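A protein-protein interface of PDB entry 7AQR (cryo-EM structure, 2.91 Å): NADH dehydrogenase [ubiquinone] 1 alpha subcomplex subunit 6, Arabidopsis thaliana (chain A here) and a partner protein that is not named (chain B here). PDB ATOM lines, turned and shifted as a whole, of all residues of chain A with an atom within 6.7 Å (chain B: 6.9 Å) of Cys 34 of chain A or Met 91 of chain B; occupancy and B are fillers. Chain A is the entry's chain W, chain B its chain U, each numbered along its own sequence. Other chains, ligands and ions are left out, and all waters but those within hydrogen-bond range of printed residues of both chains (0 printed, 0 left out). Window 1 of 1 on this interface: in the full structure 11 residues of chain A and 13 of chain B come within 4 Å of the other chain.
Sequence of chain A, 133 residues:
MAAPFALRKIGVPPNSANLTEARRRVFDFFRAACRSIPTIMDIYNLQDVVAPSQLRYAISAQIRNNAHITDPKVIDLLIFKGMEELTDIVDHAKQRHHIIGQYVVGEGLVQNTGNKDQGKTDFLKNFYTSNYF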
ATOM      1  N   PHE A  29       8.213  -3.004  15.490  1.00  0.00           N
ATOM      2  CA  PHE A  29       6.915  -2.349  15.603  1.00  0.00           C
ATOM      3  C   PHE A  29       5.806  -3.214  15.022  1.00  0.00           C
ATOM      4  O   PHE A  29       4.706  -3.288  15.582  1.00  0.00           O
ATOM      5  CB  PHE A  29       6.948  -0.988  14.912  1.00  0.00           C
ATOM      6  CG  PHE A  29       5.595  -0.482  14.513  1.00  0.00           C
ATOM      7  CD1 PHE A  29       4.705  -0.023  15.467  1.00  0.00           C
ATOM      8  CD2 PHE A  29       5.212  -0.465  13.183  1.00  0.00           C
ATOM      9  CE1 PHE A  29       3.460   0.441  15.104  1.00  0.00           C
ATOM     10  CE2 PHE A  29       3.966  -0.002  12.815  1.00  0.00           C
ATOM     11  CZ  PHE A  29       3.090   0.453  13.777  1.00  0.00           C
ATOM     12  N   PHE A  30       6.071  -3.868  13.888  1.00  0.00           N
ATOM     13  CA  PHE A  30       5.072  -4.741  13.284  1.00  0.00           C
ATOM     14  C   PHE A  30       4.736  -5.903  14.207  1.00  0.00           C
ATOM     15  O   PHE A  30       3.564  -6.262  14.375  1.00  0.00           O
ATOM     16  CB  PHE A  30       5.574  -5.247  11.932  1.00  0.00           C
ATOM     17  CG  PHE A  30       4.695  -6.290  11.307  1.00  0.00           C
ATOM     18  CD1 PHE A  30       3.497  -5.938  10.708  1.00  0.00           C
ATOM     19  CD2 PHE A  30       5.068  -7.624  11.312  1.00  0.00           C
ATOM     20  CE1 PHE A  30       2.689  -6.895  10.128  1.00  0.00           C
ATOM     21  CE2 PHE A  30       4.262  -8.585  10.734  1.00  0.00           C
ATOM     22  CZ  PHE A  30       3.073  -8.219  10.141  1.00  0.00           C
ATOM     23  N   ARG A  31       5.757  -6.502  14.824  1.00  0.00           N
ATOM     24  CA  ARG A  31       5.508  -7.593  15.761  1.00  0.00           C
ATOM     25  C   ARG A  31       4.710  -7.116  16.966  1.00  0.00           C
ATOM     26  O   ARG A  31       3.795  -7.808  17.424  1.00  0.00           O
ATOM     27  CB  ARG A  31       6.829  -8.224  16.201  1.00  0.00           C
ATOM     28  CG  ARG A  31       7.574  -8.925  15.078  1.00  0.00           C
ATOM     29  CD  ARG A  31       9.057  -9.049  15.382  1.00  0.00           C
ATOM     30  NE  ARG A  31       9.296  -9.767  16.626  1.00  0.00           N
ATOM     31  CZ  ARG A  31       9.267 -11.088  16.742  1.00  0.00           C
ATOM     32  NH1 ARG A  31       9.009 -11.867  15.706  1.00  0.00           N
ATOM     33  NH2 ARG A  31       9.501 -11.640  17.929  1.00  0.00           N
ATOM     34  N   ALA A  32       5.037  -5.932  17.493  1.00  0.00           N
ATOM     35  CA  ALA A  32       4.281  -5.400  18.623  1.00  0.00           C
ATOM     36  C   ALA A  32       2.822  -5.159  18.248  1.00  0.00           C
ATOM     37  O   ALA A  32       1.909  -5.488  19.018  1.00  0.00           O
ATOM     38  CB  ALA A  32       4.925  -4.108  19.125  1.00  0.00           C
ATOM     39  N   ALA A  33       2.584  -4.597  17.062  1.00  0.00           N
ATOM     40  CA  ALA A  33       1.217  -4.365  16.609  1.00  0.00           C
ATOM     41  C   ALA A  33       0.464  -5.678  16.443  1.00  0.00           C
ATOM     42  O   ALA A  33      -0.721  -5.776  16.783  1.00  0.00           O
ATOM     43  CB  ALA A  33       1.225  -3.576  15.298  1.00  0.00           C
ATOM     44  N   CYS A  34       1.138  -6.701  15.913  1.00  0.00           N
ATOM     45  CA  CYS A  34       0.495  -8.002  15.758  1.00  0.00           C
ATOM     46  C   CYS A  34       0.145  -8.616  17.107  1.00  0.00           C
ATOM     47  O   CYS A  34      -0.936  -9.195  17.270  1.00  0.00           O
ATOM     48  CB  CYS A  34       1.393  -8.938  14.953  1.00  0.00           C
ATOM     49  SG  CYS A  34       1.654  -8.438  13.241  1.00  0.00           S
ATOM     50  N   ARG A  35       1.042  -8.504  18.087  1.00  0.00           N
ATOM     51  CA  ARG A  35       0.698  -8.953  19.434  1.00  0.00           C
ATOM     52  C   ARG A  35      -0.401  -8.120  20.072  1.00  0.00           C
ATOM     53  O   ARG A  35      -1.066  -8.610  20.992  1.00  0.00           O
ATOM     54  CB  ARG A  35       1.923  -8.948  20.351  1.00  0.00           C
ATOM     55  CG  ARG A  35       3.159  -9.609  19.785  1.00  0.00           C
ATOM     56  CD  ARG A  35       4.013 -10.183  20.898  1.00  0.00           C
ATOM     57  NE  ARG A  35       4.992 -11.142  20.403  1.00  0.00           N
ATOM     58  CZ  ARG A  35       6.222 -10.825  20.022  1.00  0.00           C
ATOM     59  NH1 ARG A  35       6.658  -9.577  20.064  1.00  0.00           N
ATOM     60  NH2 ARG A  35       7.034 -11.784  19.588  1.00  0.00           N
ATOM     61  N   SER A  36      -0.612  -6.885  19.615  1.00  0.00           N
ATOM     62  CA  SER A  36      -1.690  -6.059  20.140  1.00  0.00           C
ATOM     63  C   SER A  36      -3.061  -6.403  19.580  1.00  0.00           C
ATOM     64  O   SER A  36      -4.060  -5.875  20.078  1.00  0.00           O
ATOM     65  CB  SER A  36      -1.408  -4.575  19.866  1.00  0.00           C
ATOM     66  OG  SER A  36      -2.485  -3.766  20.309  1.00  0.00           O
ATOM     67  N   ILE A  37      -3.135  -7.262  18.567  1.00  0.00           N
ATOM     68  CA  ILE A  37      -4.402  -7.622  17.931  1.00  0.00           C
ATOM     69  C   ILE A  37      -5.358  -8.288  18.921  1.00  0.00           C
ATOM     70  O   ILE A  37      -6.537  -7.907  18.958  1.00  0.00           O
ATOM     71  CB  ILE A  37      -4.169  -8.505  16.691  1.00  0.00           C
ATOM     72  CG1 ILE A  37      -3.408  -7.724  15.617  1.00  0.00           C
ATOM     73  CG2 ILE A  37      -5.489  -9.016  16.142  1.00  0.00           C
ATOM     74  CD1 ILE A  37      -4.172  -6.539  15.070  1.00  0.00           C
ATOM     75  N   PRO A  38      -4.934  -9.279  19.726  1.00  0.00           N
ATOM     76  CA  PRO A  38      -5.902  -9.900  20.654  1.00  0.00           C
ATOM     77  C   PRO A  38      -6.559  -8.916  21.608  1.00  0.00           C
ATOM     78  O   PRO A  38      -7.741  -9.079  21.940  1.00  0.00           O
ATOM     79  CB  PRO A  38      -5.063 -10.932  21.425  1.00  0.00           C
ATOM     80  CG  PRO A  38      -3.720 -10.950  20.812  1.00  0.00           C
ATOM     81  CD  PRO A  38      -3.696 -10.073  19.616  1.00  0.00           C
ATOM     82  N   ARG A  56      -4.150  -7.823  10.459  1.00  0.00           N
ATOM     83  CA  ARG A  56      -2.723  -8.045  10.271  1.00  0.00           C
ATOM     84  C   ARG A  56      -2.324  -7.678   8.847  1.00  0.00           C
ATOM     85  O   ARG A  56      -1.302  -7.015   8.618  1.00  0.00           O
ATOM     86  CB  ARG A  56      -2.403  -9.511  10.565  1.00  0.00           C
ATOM     87  CG  ARG A  56      -2.248  -9.835  12.048  1.00  0.00           C
ATOM     88  CD  ARG A  56      -1.486 -11.127  12.292  1.00  0.00           C
ATOM     89  NE  ARG A  56      -0.692 -11.074  13.513  1.00  0.00           N
ATOM     90  CZ  ARG A  56      -1.071 -11.618  14.663  1.00  0.00           C
ATOM     91  NH1 ARG A  56      -2.220 -12.262  14.777  1.00  0.00           N
ATOM     92  NH2 ARG A  56      -0.279 -11.510  15.727  1.00  0.00           N
ATOM     93  N   ILE A  59      -2.169  -3.756   8.563  1.00  0.00           N
ATOM     94  CA  ILE A  59      -0.882  -3.189   8.983  1.00  0.00           C
ATOM     95  C   ILE A  59       0.210  -3.524   7.973  1.00  0.00           C
ATOM     96  O   ILE A  59       1.063  -2.682   7.655  1.00  0.00           O
ATOM     97  CB  ILE A  59      -0.490  -3.623  10.411  1.00  0.00           C
ATOM     98  CG1 ILE A  59      -1.469  -3.105  11.474  1.00  0.00           C
ATOM     99  CG2 ILE A  59       0.925  -3.171  10.746  1.00  0.00           C
ATOM    100  CD1 ILE A  59      -2.631  -3.958  11.795  1.00  0.00           C
ATOM    101  N   LEU A  86      -0.963   3.151  17.610  1.00  0.00           N
ATOM    102  CA  LEU A  86      -1.227   1.855  18.224  1.00  0.00           C
ATOM    103  C   LEU A  86      -1.530   2.003  19.709  1.00  0.00           C
ATOM    104  O   LEU A  86      -2.445   1.361  20.233  1.00  0.00           O
ATOM    105  CB  LEU A  86      -0.034   0.925  18.006  1.00  0.00           C
ATOM    106  CG  LEU A  86      -0.015  -0.381  18.801  1.00  0.00           C
ATOM    107  CD1 LEU A  86      -1.245  -1.214  18.487  1.00  0.00           C
ATOM    108  CD2 LEU A  86       1.255  -1.161  18.513  1.00  0.00           C
ATOM    109  N   ASP B  85       6.815 -11.032   4.968  1.00  0.00           N
ATOM    110  CA  ASP B  85       6.254 -12.379   5.008  1.00  0.00           C
ATOM    111  C   ASP B  85       7.122 -13.318   5.836  1.00  0.00           C
ATOM    112  O   ASP B  85       6.609 -14.266   6.445  1.00  0.00           O
ATOM    113  CB  ASP B  85       6.077 -12.917   3.589  1.00  0.00           C
ATOM    114  CG  ASP B  85       5.016 -12.163   2.812  1.00  0.00           C
ATOM    115  OD1 ASP B  85       4.226 -11.432   3.444  1.00  0.00           O
ATOM    116  OD2 ASP B  85       4.972 -12.299   1.572  1.00  0.00           O
ATOM    117  N   SER B  86       8.432 -13.062   5.887  1.00  0.00           N
ATOM    118  CA  SER B  86       9.326 -13.888   6.693  1.00  0.00           C
ATOM    119  C   SER B  86       9.003 -13.769   8.177  1.00  0.00           C
ATOM    120  O   SER B  86       9.152 -14.737   8.931  1.00  0.00           O
ATOM    121  CB  SER B  86      10.779 -13.502   6.430  1.00  0.00           C
ATOM    122  OG  SER B  86      11.658 -14.255   7.246  1.00  0.00           O
ATOM    123  N   VAL B  87       8.588 -12.582   8.623  1.00  0.00           N
ATOM    124  CA  VAL B  87       8.136 -12.451  10.005  1.00  0.00           C
ATOM    125  C   VAL B  87       6.656 -12.800  10.141  1.00  0.00           C
ATOM    126  O   VAL B  87       6.214 -13.198  11.227  1.00  0.00           O
ATOM    127  CB  VAL B  87       8.426 -11.038  10.544  1.00  0.00           C
ATOM    128  CG1 VAL B  87       7.516 -10.007   9.899  1.00  0.00           C
ATOM    129  CG2 VAL B  87       8.304 -11.002  12.061  1.00  0.00           C
ATOM    130  N   GLU B  88       5.887 -12.697   9.055  1.00  0.00           N
ATOM    131  CA  GLU B  88       4.473 -13.043   9.101  1.00  0.00           C
ATOM    132  C   GLU B  88       4.271 -14.539   9.303  1.00  0.00           C
ATOM    133  O   GLU B  88       3.333 -14.951   9.987  1.00  0.00           O
ATOM    134  CB  GLU B  88       3.777 -12.574   7.823  1.00  0.00           C
ATOM    135  CG  GLU B  88       2.288 -12.882   7.775  1.00  0.00           C
ATOM    136  CD  GLU B  88       1.494 -12.110   8.810  1.00  0.00           C
ATOM    137  OE1 GLU B  88       1.931 -11.008   9.196  1.00  0.00           O
ATOM    138  OE2 GLU B  88       0.433 -12.609   9.237  1.00  0.00           O
ATOM    139  N   VAL B  89       5.131 -15.371   8.708  1.00  0.00           N
ATOM    140  CA  VAL B  89       5.012 -16.812   8.929  1.00  0.00           C
ATOM    141  C   VAL B  89       5.259 -17.148  10.398  1.00  0.00           C
ATOM    142  O   VAL B  89       4.531 -17.949  10.999  1.00  0.00           O
ATOM    143  CB  VAL B  89       5.952 -17.597   7.989  1.00  0.00           C
ATOM    144  CG1 VAL B  89       5.581 -17.351   6.542  1.00  0.00           C
ATOM    145  CG2 VAL B  89       7.410 -17.236   8.220  1.00  0.00           C
ATOM    146  N   VAL B  90       6.271 -16.522  11.004  1.00  0.00           N
ATOM    147  CA  VAL B  90       6.565 -16.763  12.415  1.00  0.00           C
ATOM    148  C   VAL B  90       5.409 -16.282  13.282  1.00  0.00           C
ATOM    149  O   VAL B  90       5.018 -16.941  14.253  1.00  0.00           O
ATOM    150  CB  VAL B  90       7.889 -16.082  12.808  1.00  0.00           C
ATOM    151  CG1 VAL B  90       8.153 -16.247  14.296  1.00  0.00           C
ATOM    152  CG2 VAL B  90       9.039 -16.643  11.986  1.00  0.00           C
ATOM    153  N   MET B  91       4.849 -15.118  12.947  1.00  0.00           N
ATOM    154  CA  MET B  91       3.729 -14.588  13.714  1.00  0.00           C
ATOM    155  C   MET B  91       2.488 -15.462  13.559  1.00  0.00           C
ATOM    156  O   MET B  91       1.692 -15.597  14.495  1.00  0.00           O
ATOM    157  CB  MET B  91       3.450 -13.147  13.289  1.00  0.00           C
ATOM    158  CG  MET B  91       2.383 -12.452  14.104  1.00  0.00           C
ATOM    159  SD  MET B  91       2.876 -12.286  15.829  1.00  0.00           S
ATOM    160  CE  MET B  91       4.136 -11.025  15.714  1.00  0.00           C
ATOM    161  N   ALA B  92       2.299 -16.053  12.378  1.00  0.00           N
ATOM    162  CA  ALA B  92       1.209 -17.002  12.186  1.00  0.00           C
ATOM    163  C   ALA B  92       1.440 -18.267  12.998  1.00  0.00           C
ATOM    164  O   ALA B  92       0.484 -18.917  13.439  1.00  0.00           O
ATOM    165  CB  ALA B  92       1.053 -17.333  10.702  1.00  0.00           C
ATOM    166  N   LEU B  93       2.707 -18.642  13.196  1.00  0.00           N
ATOM    167  CA  LEU B  93       3.012 -19.774  14.065  1.00  0.00           C
ATOM    168  C   LEU B  93       2.535 -19.515  15.489  1.00  0.00           C
ATOM    169  O   LEU B  93       2.094 -20.439  16.183  1.00  0.00           O
ATOM    170  CB  LEU B  93       4.513 -20.068  14.043  1.00  0.00           C
ATOM    171  CG  LEU B  93       5.069 -20.648  12.742  1.00  0.00           C
ATOM    172  CD1 LEU B  93       6.512 -21.094  12.927  1.00  0.00           C
ATOM    173  CD2 LEU B  93       4.207 -21.800  12.256  1.00  0.00           C
ATOM    174  N   GLU B  94       2.616 -18.265  15.943  1.00  0.00           N
ATOM    175  CA  GLU B  94       2.054 -17.868  17.227  1.00  0.00           C
ATOM    176  C   GLU B  94       0.661 -17.268  17.089  1.00  0.00           C
ATOM    177  O   GLU B  94       0.109 -16.772  18.076  1.00  0.00           O
ATOM    178  CB  GLU B  94       2.983 -16.885  17.942  1.00  0.00           C
ATOM    179  CG  GLU B  94       3.479 -15.736  17.088  1.00  0.00           C
ATOM    180  CD  GLU B  94       4.568 -14.930  17.768  1.00  0.00           C
ATOM    181  OE1 GLU B  94       4.795 -15.137  18.979  1.00  0.00           O
ATOM    182  OE2 GLU B  94       5.202 -14.095  17.090  1.00  0.00           O
ATOM    183  N   GLU B  95       0.086 -17.289  15.884  1.00  0.00           N
ATOM    184  CA  GLU B  95      -1.316 -16.954  15.685  1.00  0.00           C
ATOM    185  C   GLU B  95      -2.225 -18.170  15.723  1.00  0.00           C
ATOM    186  O   GLU B  95      -3.408 -18.030  16.048  1.00  0.00           O
ATOM    187  CB  GLU B  95      -1.508 -16.220  14.348  1.00  0.00           C
ATOM    188  CG  GLU B  95      -2.874 -15.577  14.165  1.00  0.00           C
ATOM    189  CD  GLU B  95      -2.981 -14.792  12.870  1.00  0.00           C
ATOM    190  OE1 GLU B  95      -1.989 -14.751  12.113  1.00  0.00           O
ATOM    191  OE2 GLU B  95      -4.059 -14.219  12.609  1.00  0.00           O
ATOM    192  N   GLU B  96      -1.703 -19.353  15.409  1.00  0.00           N
ATOM    193  CA  GLU B  96      -2.435 -20.603  15.548  1.00  0.00           C
ATOM    194  C   GLU B  96      -2.242 -21.247  16.915  1.00  0.00           C
ATOM    195  O   GLU B  96      -2.806 -22.316  17.168  1.00  0.00           O
ATOM    196  CB  GLU B  96      -2.025 -21.576  14.431  1.00  0.00           C
ATOM    197  CG  GLU B  96      -0.545 -21.953  14.408  1.00  0.00           C
ATOM    198  CD  GLU B  96      -0.208 -23.132  15.301  1.00  0.00           C
ATOM    199  OE1 GLU B  96      -1.128 -23.901  15.651  1.00  0.00           O
ATOM    200  OE2 GLU B  96       0.980 -23.290  15.651  1.00  0.00           O
ATOM    201  N   PHE B  97      -1.468 -20.619  17.800  1.00  0.00           N
ATOM    202  CA  PHE B  97      -1.305 -21.086  19.169  1.00  0.00           C
ATOM    203  C   PHE B  97      -1.049 -19.875  20.059  1.00  0.00           C
ATOM    204  O   PHE B  97      -1.094 -18.729  19.608  1.00  0.00           O
ATOM    205  CB  PHE B  97      -0.182 -22.123  19.274  1.00  0.00           C
ATOM    206  CG  PHE B  97      -0.360 -23.089  20.411  1.00  0.00           C
ATOM    207  CD1 PHE B  97      -1.311 -24.093  20.340  1.00  0.00           C
ATOM    208  CD2 PHE B  97       0.422 -22.994  21.552  1.00  0.00           C
ATOM    209  CE1 PHE B  97      -1.481 -24.981  21.382  1.00  0.00           C
ATOM    210  CE2 PHE B  97       0.257 -23.879  22.598  1.00  0.00           C
ATOM    211  CZ  PHE B  97      -0.697 -24.872  22.513  1.00  0.00           C
ATOM    212  N   ILE B 101       7.378 -16.181  20.435  1.00  0.00           N
ATOM    213  CA  ILE B 101       8.714 -16.295  19.862  1.00  0.00           C
ATOM    214  C   ILE B 101       9.471 -15.010  20.188  1.00  0.00           C
ATOM    215  O   ILE B 101       9.046 -13.921  19.771  1.00  0.00           O
ATOM    216  CB  ILE B 101       8.668 -16.541  18.346  1.00  0.00           C
ATOM    217  CG1 ILE B 101       8.030 -17.897  18.031  1.00  0.00           C
ATOM    218  CG2 ILE B 101      10.067 -16.451  17.753  1.00  0.00           C
ATOM    219  CD1 ILE B 101       6.545 -17.830  17.764  1.00  0.00           C
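The guanidinium group of Arg 56 of chain A is in hydrogen-bond range of the side-chain sulfur of Met 91 of chain B (3.3 Å). The guanidinium group of Arg 35 of chain A is in salt-bridge range of the side-chain carboxylate of Glu 94 of chain B, at 3.9 Å. NH1 of Arg 56 of chain A is in salt-bridge range of OE2 of Glu 95 of chain B (3.5 Å). NH2 of Arg 31 of chain A lies within hydrogen-bond range of O of Ile 101 of chain B. O of Ile 101 of chain B is in hydrogen-bond range of NH2 of Arg 35 of chain A (2.9 Å).
OE1 of Glu 94 of chain B is in hydrogen-bond range of N of Ile 101 of chain B, at 3.1 Å. O of Phe 30 of chain A lies within hydrogen-bond range of SG of Cys 34 of chain A. The backbone carbonyl oxygen of Cys 34 of chain A lies within hydrogen-bond range of the guanidinium group of Arg 56 of chain A.
Among the printed residues, merely in contact across the chains: Phe 30 of chain A with Val 87 of chain B (3.6 Å), Phe 30 of chain A with Glu 88 of chain B (3.2 Å), Arg 31 of chain A with Val 87 of chain B (3.7 Å), Arg 31 of chain A with Met 91 of chain B (3.7 Å), Cys 34 of chain A with Met 91 of chain B (3.5 Å) and Arg 56 of chain A with Glu 88 of chain B (3.9 Å).
Of chain B, only Met 91 comes within 4 Å of Cys 34 of chain A. Met 91 of chain B touches just these residues of chain A: Arg 31, Cys 34 and Arg 56. Of the printed residues of chain A, Glu 88 of chain B touches Phe 30 (3.2 Å) and Arg 56 (3.9 Å). Printed residues of chain B within 4 Å of Arg 31 of chain A: Val 87, Met 91 and Ile 101. Of the printed residues of chain B, Phe 30 of chain A touches Val 87 and Glu 88. Of the printed residues of chain A, Val 87 of chain B touches Phe 30 (3.6 Å) and Arg 31 (3.7 Å). Of the printed residues of chain A, Glu 94 of chain B touches Arg 35. Ile 37 of chain A touches none of the printed residues of chain B. Ala 33 of chain A touches none of the printed residues of chain B. The nearest residue of chain B that does not touch Cys 34 of chain A is Glu 88 of chain B (4.8 Å). The nearest printed residue of chain B that does not touch Arg 56 of chain A is Glu 94 of chain B (5.8 Å).
Printed residues of chain B that touch a printed residue of chain A: Val 87, Glu 88, Met 91, Glu 94, Glu 95 and Ile 101. Among the printed residues, Asp or Glu carboxylates within 4 Å of a Lys or Arg side-chain nitrogen of the other chain: Arg 35 of chain A with Glu 94 of chain B (3.9 Å) and Arg 56 of chain A with Glu 95 of chain B (3.5 Å).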
